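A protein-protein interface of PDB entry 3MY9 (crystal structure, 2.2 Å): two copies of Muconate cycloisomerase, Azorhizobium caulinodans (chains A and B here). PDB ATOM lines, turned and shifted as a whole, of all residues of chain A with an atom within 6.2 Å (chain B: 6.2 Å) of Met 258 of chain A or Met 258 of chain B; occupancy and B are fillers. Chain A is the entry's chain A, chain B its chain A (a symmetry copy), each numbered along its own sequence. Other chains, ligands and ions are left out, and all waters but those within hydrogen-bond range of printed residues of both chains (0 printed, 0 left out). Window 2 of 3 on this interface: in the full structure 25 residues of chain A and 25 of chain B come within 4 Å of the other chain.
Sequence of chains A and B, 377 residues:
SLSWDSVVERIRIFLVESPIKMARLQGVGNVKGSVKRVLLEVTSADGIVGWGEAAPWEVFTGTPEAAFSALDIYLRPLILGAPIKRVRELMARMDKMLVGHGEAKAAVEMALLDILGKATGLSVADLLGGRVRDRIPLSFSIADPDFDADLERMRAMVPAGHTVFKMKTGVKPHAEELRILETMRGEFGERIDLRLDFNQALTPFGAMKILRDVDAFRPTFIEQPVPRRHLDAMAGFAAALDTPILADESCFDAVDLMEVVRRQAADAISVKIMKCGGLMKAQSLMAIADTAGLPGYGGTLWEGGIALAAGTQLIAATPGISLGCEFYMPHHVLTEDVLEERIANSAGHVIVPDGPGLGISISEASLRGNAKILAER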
ATOM      1  N   ASP A 253       7.937  -1.532  -1.151  1.00  0.00           N
ATOM      2  CA  ASP A 253       7.071  -1.743   0.021  1.00  0.00           C
ATOM      3  C   ASP A 253       7.863  -2.299   1.201  1.00  0.00           C
ATOM      4  O   ASP A 253       9.087  -2.502   1.114  1.00  0.00           O
ATOM      5  CB  ASP A 253       5.869  -2.649  -0.345  1.00  0.00           C
ATOM      6  CG  ASP A 253       6.282  -4.074  -0.776  1.00  0.00           C
ATOM      7  OD1 ASP A 253       7.443  -4.469  -0.573  1.00  0.00           O
ATOM      8  OD2 ASP A 253       5.427  -4.812  -1.320  1.00  0.00           O
ATOM      9  N   ALA A 254       7.166  -2.532   2.302  1.00  0.00           N
ATOM     10  CA  ALA A 254       7.796  -2.917   3.552  1.00  0.00           C
ATOM     11  C   ALA A 254       8.478  -4.266   3.386  1.00  0.00           C
ATOM     12  O   ALA A 254       9.601  -4.465   3.874  1.00  0.00           O
ATOM     13  CB  ALA A 254       6.776  -2.948   4.677  1.00  0.00           C
ATOM     14  N   VAL A 255       7.843  -5.174   2.663  1.00  0.00           N
ATOM     15  CA  VAL A 255       8.452  -6.463   2.392  1.00  0.00           C
ATOM     16  C   VAL A 255       9.803  -6.358   1.656  1.00  0.00           C
ATOM     17  O   VAL A 255      10.770  -7.025   2.031  1.00  0.00           O
ATOM     18  CB  VAL A 255       7.514  -7.374   1.572  1.00  0.00           C
ATOM     19  CG1 VAL A 255       8.229  -8.675   1.253  1.00  0.00           C
ATOM     20  CG2 VAL A 255       6.210  -7.637   2.330  1.00  0.00           C
ATOM     21  N   ASP A 256       9.866  -5.541   0.602  1.00  0.00           N
ATOM     22  CA  ASP A 256      11.115  -5.357  -0.116  1.00  0.00           C
ATOM     23  C   ASP A 256      12.155  -4.789   0.866  1.00  0.00           C
ATOM     24  O   ASP A 256      13.314  -5.182   0.845  1.00  0.00           O
ATOM     25  CB  ASP A 256      10.982  -4.368  -1.310  1.00  0.00           C
ATOM     26  CG  ASP A 256      10.068  -4.875  -2.424  1.00  0.00           C
ATOM     27  OD1 ASP A 256       9.788  -6.081  -2.518  1.00  0.00           O
ATOM     28  OD2 ASP A 256       9.631  -4.042  -3.246  1.00  0.00           O
ATOM     29  N   LEU A 257      11.743  -3.848   1.692  1.00  0.00           N
ATOM     30  CA  LEU A 257      12.670  -3.166   2.557  1.00  0.00           C
ATOM     31  C   LEU A 257      13.297  -4.157   3.526  1.00  0.00           C
ATOM     32  O   LEU A 257      14.505  -4.148   3.683  1.00  0.00           O
ATOM     33  CB  LEU A 257      12.009  -2.007   3.298  1.00  0.00           C
ATOM     34  CG  LEU A 257      12.910  -1.239   4.290  1.00  0.00           C
ATOM     35  CD1 LEU A 257      14.140  -0.637   3.598  1.00  0.00           C
ATOM     36  CD2 LEU A 257      12.092  -0.169   4.978  1.00  0.00           C
ATOM     37  N   MET A 258      12.509  -5.042   4.133  1.00  0.00           N
ATOM     38  CA  MET A 258      13.100  -6.061   5.020  1.00  0.00           C
ATOM     39  C   MET A 258      14.155  -6.919   4.328  1.00  0.00           C
ATOM     40  O   MET A 258      15.160  -7.284   4.936  1.00  0.00           O
ATOM     41  CB  MET A 258      12.043  -6.957   5.699  1.00  0.00           C
ATOM     42  CG  MET A 258      11.263  -6.220   6.819  1.00  0.00           C
ATOM     43  SD  MET A 258      12.127  -5.650   8.346  1.00  0.00           S
ATOM     44  CE  MET A 258      13.847  -5.664   7.977  1.00  0.00           C
ATOM     45  N   GLU A 259      13.945  -7.221   3.048  1.00  0.00           N
ATOM     46  CA  GLU A 259      14.945  -7.984   2.294  1.00  0.00           C
ATOM     47  C   GLU A 259      16.170  -7.127   1.938  1.00  0.00           C
ATOM     48  O   GLU A 259      17.296  -7.612   1.957  1.00  0.00           O
ATOM     49  CB  GLU A 259      14.321  -8.578   1.049  1.00  0.00           C
ATOM     50  CG  GLU A 259      15.211  -9.604   0.374  1.00  0.00           C
ATOM     51  CD  GLU A 259      15.461 -10.859   1.231  1.00  0.00           C
ATOM     52  OE1 GLU A 259      14.608 -11.267   2.055  1.00  0.00           O
ATOM     53  OE2 GLU A 259      16.545 -11.442   1.070  1.00  0.00           O
ATOM     54  N   VAL A 260      15.951  -5.859   1.611  1.00  0.00           N
ATOM     55  CA  VAL A 260      17.038  -4.950   1.355  1.00  0.00           C
ATOM     56  C   VAL A 260      17.918  -4.846   2.626  1.00  0.00           C
ATOM     57  O   VAL A 260      19.137  -4.883   2.529  1.00  0.00           O
ATOM     58  CB  VAL A 260      16.509  -3.571   0.884  1.00  0.00           C
ATOM     59  CG1 VAL A 260      17.562  -2.473   0.950  1.00  0.00           C
ATOM     60  CG2 VAL A 260      15.907  -3.690  -0.547  1.00  0.00           C
ATOM     61  N   VAL A 261      17.299  -4.694   3.800  1.00  0.00           N
ATOM     62  CA  VAL A 261      18.052  -4.596   5.041  1.00  0.00           C
ATOM     63  C   VAL A 261      18.824  -5.879   5.276  1.00  0.00           C
ATOM     64  O   VAL A 261      19.998  -5.841   5.559  1.00  0.00           O
ATOM     65  CB  VAL A 261      17.146  -4.312   6.240  1.00  0.00           C
ATOM     66  CG1 VAL A 261      17.918  -4.362   7.554  1.00  0.00           C
ATOM     67  CG2 VAL A 261      16.439  -2.968   6.055  1.00  0.00           C
ATOM     68  N   ARG A 262      18.153  -7.012   5.115  1.00  0.00           N
ATOM     69  CA  ARG A 262      18.738  -8.321   5.401  1.00  0.00           C
ATOM     70  C   ARG A 262      19.947  -8.597   4.534  1.00  0.00           C
ATOM     71  O   ARG A 262      20.903  -9.246   4.977  1.00  0.00           O
ATOM     72  CB  ARG A 262      17.695  -9.389   5.126  1.00  0.00           C
ATOM     73  CG  ARG A 262      18.137 -10.804   5.414  1.00  0.00           C
ATOM     74  CD  ARG A 262      17.013 -11.816   5.102  1.00  0.00           C
ATOM     75  NE  ARG A 262      17.566 -13.162   5.028  1.00  0.00           N
ATOM     76  CZ  ARG A 262      18.217 -13.670   3.978  1.00  0.00           C
ATOM     77  NH1 ARG A 262      18.376 -12.962   2.873  1.00  0.00           N
ATOM     78  NH2 ARG A 262      18.698 -14.915   4.043  1.00  0.00           N
ATOM     79  N   ARG A 263      19.878  -8.151   3.278  1.00  0.00           N
ATOM     80  CA  ARG A 263      20.964  -8.368   2.337  1.00  0.00           C
ATOM     81  C   ARG A 263      21.934  -7.175   2.337  1.00  0.00           C
ATOM     82  O   ARG A 263      22.946  -7.227   1.657  1.00  0.00           O
ATOM     83  CB  ARG A 263      20.426  -8.572   0.911  1.00  0.00           C
ATOM     84  CG  ARG A 263      19.434  -9.709   0.757  1.00  0.00           C
ATOM     85  CD  ARG A 263      20.093 -11.043   0.488  1.00  0.00           C
ATOM     86  NE  ARG A 263      20.139 -11.345  -0.944  1.00  0.00           N
ATOM     87  CZ  ARG A 263      19.103 -11.750  -1.671  1.00  0.00           C
ATOM     88  NH1 ARG A 263      19.272 -11.988  -2.954  1.00  0.00           N
ATOM     89  NH2 ARG A 263      17.892 -11.891  -1.135  1.00  0.00           N
ATOM     90  N   ILE A 288      10.750   0.946   9.829  1.00  0.00           N
ATOM     91  CA  ILE A 288      11.721  -0.078   9.568  1.00  0.00           C
ATOM     92  C   ILE A 288      13.064   0.554   9.155  1.00  0.00           C
ATOM     93  O   ILE A 288      14.110   0.176   9.677  1.00  0.00           O
ATOM     94  CB  ILE A 288      11.285  -1.039   8.466  1.00  0.00           C
ATOM     95  CG1 ILE A 288      10.032  -1.800   8.877  1.00  0.00           C
ATOM     96  CG2 ILE A 288      12.408  -2.029   8.156  1.00  0.00           C
ATOM     97  CD1 ILE A 288       9.319  -2.409   7.729  1.00  0.00           C
ATOM     98  N   THR A 291      14.975   2.395  12.032  1.00  0.00           N
ATOM     99  CA  THR A 291      15.626   1.409  12.872  1.00  0.00           C
ATOM    100  C   THR A 291      16.873   0.851  12.180  1.00  0.00           C
ATOM    101  O   THR A 291      17.913   0.685  12.803  1.00  0.00           O
ATOM    102  CB  THR A 291      14.654   0.276  13.263  1.00  0.00           C
ATOM    103  OG1 THR A 291      13.471   0.858  13.811  1.00  0.00           O
ATOM    104  CG2 THR A 291      15.287  -0.639  14.310  1.00  0.00           C
ATOM    105  N   ALA A 292      16.786   0.629  10.877  1.00  0.00           N
ATOM    106  CA  ALA A 292      17.895   0.056  10.115  1.00  0.00           C
ATOM    107  C   ALA A 292      18.961   1.056   9.692  1.00  0.00           C
ATOM    108  O   ALA A 292      19.971   0.649   9.154  1.00  0.00           O
ATOM    109  CB  ALA A 292      17.392  -0.677   8.876  1.00  0.00           C
ATOM    110  N   ASP B 253      12.386  -2.995  22.591  1.00  0.00           N
ATOM    111  CA  ASP B 253      12.339  -1.867  21.646  1.00  0.00           C
ATOM    112  C   ASP B 253      12.566  -2.335  20.212  1.00  0.00           C
ATOM    113  O   ASP B 253      12.742  -3.539  19.951  1.00  0.00           O
ATOM    114  CB  ASP B 253      13.349  -0.767  22.060  1.00  0.00           C
ATOM    115  CG  ASP B 253      14.820  -1.237  22.021  1.00  0.00           C
ATOM    116  OD1 ASP B 253      15.113  -2.304  21.455  1.00  0.00           O
ATOM    117  OD2 ASP B 253      15.698  -0.521  22.560  1.00  0.00           O
ATOM    118  N   ALA B 254      12.553  -1.387  19.289  1.00  0.00           N
ATOM    119  CA  ALA B 254      12.603  -1.687  17.869  1.00  0.00           C
ATOM    120  C   ALA B 254      13.927  -2.355  17.535  1.00  0.00           C
ATOM    121  O   ALA B 254      13.963  -3.321  16.757  1.00  0.00           O
ATOM    122  CB  ALA B 254      12.399  -0.425  17.049  1.00  0.00           C
ATOM    123  N   VAL B 255      15.005  -1.892  18.147  1.00  0.00           N
ATOM    124  CA  VAL B 255      16.298  -2.517  17.944  1.00  0.00           C
ATOM    125  C   VAL B 255      16.326  -4.008  18.336  1.00  0.00           C
ATOM    126  O   VAL B 255      16.849  -4.839  17.589  1.00  0.00           O
ATOM    127  CB  VAL B 255      17.413  -1.783  18.720  1.00  0.00           C
ATOM    128  CG1 VAL B 255      18.726  -2.522  18.533  1.00  0.00           C
ATOM    129  CG2 VAL B 255      17.532  -0.329  18.257  1.00  0.00           C
ATOM    130  N   ASP B 256      15.785  -4.344  19.509  1.00  0.00           N
ATOM    131  CA  ASP B 256      15.734  -5.734  19.928  1.00  0.00           C
ATOM    132  C   ASP B 256      14.910  -6.519  18.893  1.00  0.00           C
ATOM    133  O   ASP B 256      15.255  -7.639  18.538  1.00  0.00           O
ATOM    134  CB  ASP B 256      15.067  -5.918  21.322  1.00  0.00           C
ATOM    135  CG  ASP B 256      15.859  -5.288  22.466  1.00  0.00           C
ATOM    136  OD1 ASP B 256      17.062  -5.010  22.330  1.00  0.00           O
ATOM    137  OD2 ASP B 256      15.265  -5.084  23.546  1.00  0.00           O
ATOM    138  N   LEU B 257      13.814  -5.942  18.442  1.00  0.00           N
ATOM    139  CA  LEU B 257      12.911  -6.649  17.572  1.00  0.00           C
ATOM    140  C   LEU B 257      13.618  -6.999  16.270  1.00  0.00           C
ATOM    141  O   LEU B 257      13.528  -8.133  15.834  1.00  0.00           O
ATOM    142  CB  LEU B 257      11.632  -5.857  17.315  1.00  0.00           C
ATOM    143  CG  LEU B 257      10.617  -6.510  16.351  1.00  0.00           C
ATOM    144  CD1 LEU B 257      10.156  -7.885  16.852  1.00  0.00           C
ATOM    145  CD2 LEU B 257       9.443  -5.577  16.160  1.00  0.00           C
ATOM    146  N   MET B 258      14.357  -6.066  15.675  1.00  0.00           N
ATOM    147  CA  MET B 258      15.112  -6.399  14.452  1.00  0.00           C
ATOM    148  C   MET B 258      16.073  -7.569  14.642  1.00  0.00           C
ATOM    149  O   MET B 258      16.245  -8.388  13.740  1.00  0.00           O
ATOM    150  CB  MET B 258      15.855  -5.188  13.852  1.00  0.00           C
ATOM    151  CG  MET B 258      14.899  -4.178  13.165  1.00  0.00           C
ATOM    152  SD  MET B 258      13.948  -4.662  11.660  1.00  0.00           S
ATOM    153  CE  MET B 258      13.989  -6.418  11.590  1.00  0.00           C
ATOM    154  N   GLU B 259      16.681  -7.668  15.823  1.00  0.00           N
ATOM    155  CA  GLU B 259      17.567  -8.801  16.107  1.00  0.00           C
ATOM    156  C   GLU B 259      16.778 -10.097  16.354  1.00  0.00           C
ATOM    157  O   GLU B 259      17.204 -11.173  15.948  1.00  0.00           O
ATOM    158  CB  GLU B 259      18.465  -8.482  17.283  1.00  0.00           C
ATOM    159  CG  GLU B 259      19.591  -9.484  17.455  1.00  0.00           C
ATOM    160  CD  GLU B 259      20.593  -9.488  16.286  1.00  0.00           C
ATOM    161  OE1 GLU B 259      20.821  -8.452  15.618  1.00  0.00           O
ATOM    162  OE2 GLU B 259      21.159 -10.564  16.035  1.00  0.00           O
ATOM    163  N   VAL B 260      15.634  -9.994  17.020  1.00  0.00           N
ATOM    164  CA  VAL B 260      14.776 -11.133  17.219  1.00  0.00           C
ATOM    165  C   VAL B 260      14.338 -11.682  15.838  1.00  0.00           C
ATOM    166  O   VAL B 260      14.354 -12.887  15.627  1.00  0.00           O
ATOM    167  CB  VAL B 260      13.571 -10.767  18.123  1.00  0.00           C
ATOM    168  CG1 VAL B 260      12.452 -11.801  18.074  1.00  0.00           C
ATOM    169  CG2 VAL B 260      14.051 -10.527  19.584  1.00  0.00           C
ATOM    170  N   VAL B 261      13.931 -10.801  14.920  1.00  0.00           N
ATOM    171  CA  VAL B 261      13.510 -11.234  13.596  1.00  0.00           C
ATOM    172  C   VAL B 261      14.671 -11.895  12.879  1.00  0.00           C
ATOM    173  O   VAL B 261      14.524 -12.966  12.340  1.00  0.00           O
ATOM    174  CB  VAL B 261      12.978 -10.072  12.756  1.00  0.00           C
ATOM    175  CG1 VAL B 261      12.684 -10.502  11.323  1.00  0.00           C
ATOM    176  CG2 VAL B 261      11.744  -9.464  13.425  1.00  0.00           C
ATOM    177  N   ARG B 262      15.832 -11.255  12.918  1.00  0.00           N
ATOM    178  CA  ARG B 262      17.012 -11.720  12.192  1.00  0.00           C
ATOM    179  C   ARG B 262      17.446 -13.097  12.650  1.00  0.00           C
ATOM    180  O   ARG B 262      17.935 -13.901  11.846  1.00  0.00           O
ATOM    181  CB  ARG B 262      18.151 -10.749  12.443  1.00  0.00           C
ATOM    182  CG  ARG B 262      19.439 -11.074  11.723  1.00  0.00           C
ATOM    183  CD  ARG B 262      20.536 -10.034  12.042  1.00  0.00           C
ATOM    184  NE  ARG B 262      21.839 -10.555  11.654  1.00  0.00           N
ATOM    185  CZ  ARG B 262      22.562 -11.428  12.361  1.00  0.00           C
ATOM    186  NH1 ARG B 262      22.135 -11.867  13.533  1.00  0.00           N
ATOM    187  NH2 ARG B 262      23.737 -11.849  11.883  1.00  0.00           N
ATOM    188  N   ARG B 263      17.318 -13.344  13.955  1.00  0.00           N
ATOM    189  CA  ARG B 263      17.716 -14.620  14.525  1.00  0.00           C
ATOM    190  C   ARG B 263      16.524 -15.590  14.580  1.00  0.00           C
ATOM    191  O   ARG B 263      16.702 -16.735  14.964  1.00  0.00           O
ATOM    192  CB  ARG B 263      18.275 -14.438  15.946  1.00  0.00           C
ATOM    193  CG  ARG B 263      19.451 -13.485  16.054  1.00  0.00           C
ATOM    194  CD  ARG B 263      20.786 -14.157  15.826  1.00  0.00           C
ATOM    195  NE  ARG B 263      21.422 -14.541  17.088  1.00  0.00           N
ATOM    196  CZ  ARG B 263      22.026 -13.701  17.922  1.00  0.00           C
ATOM    197  NH1 ARG B 263      22.560 -14.170  19.031  1.00  0.00           N
ATOM    198  NH2 ARG B 263      22.077 -12.394  17.676  1.00  0.00           N
ATOM    199  N   ILE B 288       7.242  -3.129  12.192  1.00  0.00           N
ATOM    200  CA  ILE B 288       8.263  -4.109  11.956  1.00  0.00           C
ATOM    201  C   ILE B 288       7.702  -5.526  12.174  1.00  0.00           C
ATOM    202  O   ILE B 288       7.906  -6.406  11.341  1.00  0.00           O
ATOM    203  CB  ILE B 288       9.476  -3.928  12.864  1.00  0.00           C
ATOM    204  CG1 ILE B 288      10.160  -2.595  12.596  1.00  0.00           C
ATOM    205  CG2 ILE B 288      10.471  -5.068  12.646  1.00  0.00           C
ATOM    206  CD1 ILE B 288      11.051  -2.166  13.699  1.00  0.00           C
ATOM    207  N   THR B 291       5.157  -6.729   9.456  1.00  0.00           N
ATOM    208  CA  THR B 291       5.888  -7.133   8.271  1.00  0.00           C
ATOM    209  C   THR B 291       6.552  -8.497   8.487  1.00  0.00           C
ATOM    210  O   THR B 291       6.525  -9.350   7.610  1.00  0.00           O
ATOM    211  CB  THR B 291       6.927  -6.069   7.863  1.00  0.00           C
ATOM    212  OG1 THR B 291       6.273  -4.802   7.773  1.00  0.00           O
ATOM    213  CG2 THR B 291       7.540  -6.407   6.505  1.00  0.00           C
ATOM    214  N   ALA B 292       7.083  -8.722   9.679  1.00  0.00           N
ATOM    215  CA  ALA B 292       7.782  -9.968   9.989  1.00  0.00           C
ATOM    216  C   ALA B 292       6.876 -11.129  10.373  1.00  0.00           C
ATOM    217  O   ALA B 292       7.365 -12.229  10.537  1.00  0.00           O
ATOM    218  CB  ALA B 292       8.810  -9.762  11.098  1.00  0.00           C
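Ala 254 of chain A touches Thr 291 of chain B (CB to OG1, 3.6 Å). Met 258 of chain B touches Met 258 of chain A (CE to CE, 3.7 Å). Met 258 of chain A touches Thr 291 of chain B (CG to CG2, 3.7 Å). CG1 of Ile 288 of chain B touches CG1 of Ile 288 of chain A (3.8 Å). Ile 288 of chain A touches Thr 291 of chain B (CD1 to OG1, 3.9 Å). Ala 254 of chain B touches Thr 291 of chain A. CG2 of Thr 291 of chain A touches CG of Met 258 of chain B, at 3.7 Å. CD1 of Ile 288 of chain B touches OG1 of Thr 291 of chain A, 3.9 Å away.
Of the 14 printed residues of chain A, 4 touch a printed residue of chain B. Printed residues of chain A that touch a printed residue of chain B: Ala 254, Met 258, Ile 288 and Thr 291. Along chain A the printed residues that touch a printed residue of chain B span positions 254 to 291. Hydrophobic or aromatic side chains of chain B that line the printed part of chain A: Ala 254, Met 258 and Ile 288. Among the printed residues, 8 pairs touch across the chains. Among the printed residues, no Asp or Glu carboxylate lies within 4 Å of a Lys or Arg side-chain nitrogen of the other chain.
Met 258 of chain A touches its own counterpart, Met 258 of chain B. Met 258 of chain A touches Thr 291 of chain B, and with the chains exchanged Thr 291 of chain A touches Met 258 of chain B. Ile 288 of chain A touches its own counterpart, Ile 288 of chain B. Ile 288 of chain A touches Thr 291 of chain B, and with the chains exchanged Thr 291 of chain A touches Ile 288 of chain B. Of the 8 pairs that touch across the chains among the printed residues, 8 have their exchanged pair printed and touching as well.
Met 258 of chain A touches two residues of chain B. Met 258 of chain B touches just these residues of chain A: Met 258 and Thr 291. Printed residues of chain A within 4 Å of Ile 288 of chain B: Ile 288 and Thr 291. Of the printed residues of chain B, Ile 288 of chain A touches Ile 288 (3.8 Å) and Thr 291 (3.9 Å). Printed residues of chain B within 4 Å of Ala 254 of chain A: Thr 291 (3.6 Å). Arg 262 of chain B touches none of the printed residues of chain A. Val 261 of chain A touches none of the printed residues of chain B. The nearest residue of chain B that does not touch Met 258 of chain A is Ile 288 of chain B (4.6 Å). The nearest printed residue of chain A that does not touch Ile 288 of chain B is Met 258 of chain A (4.6 Å).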
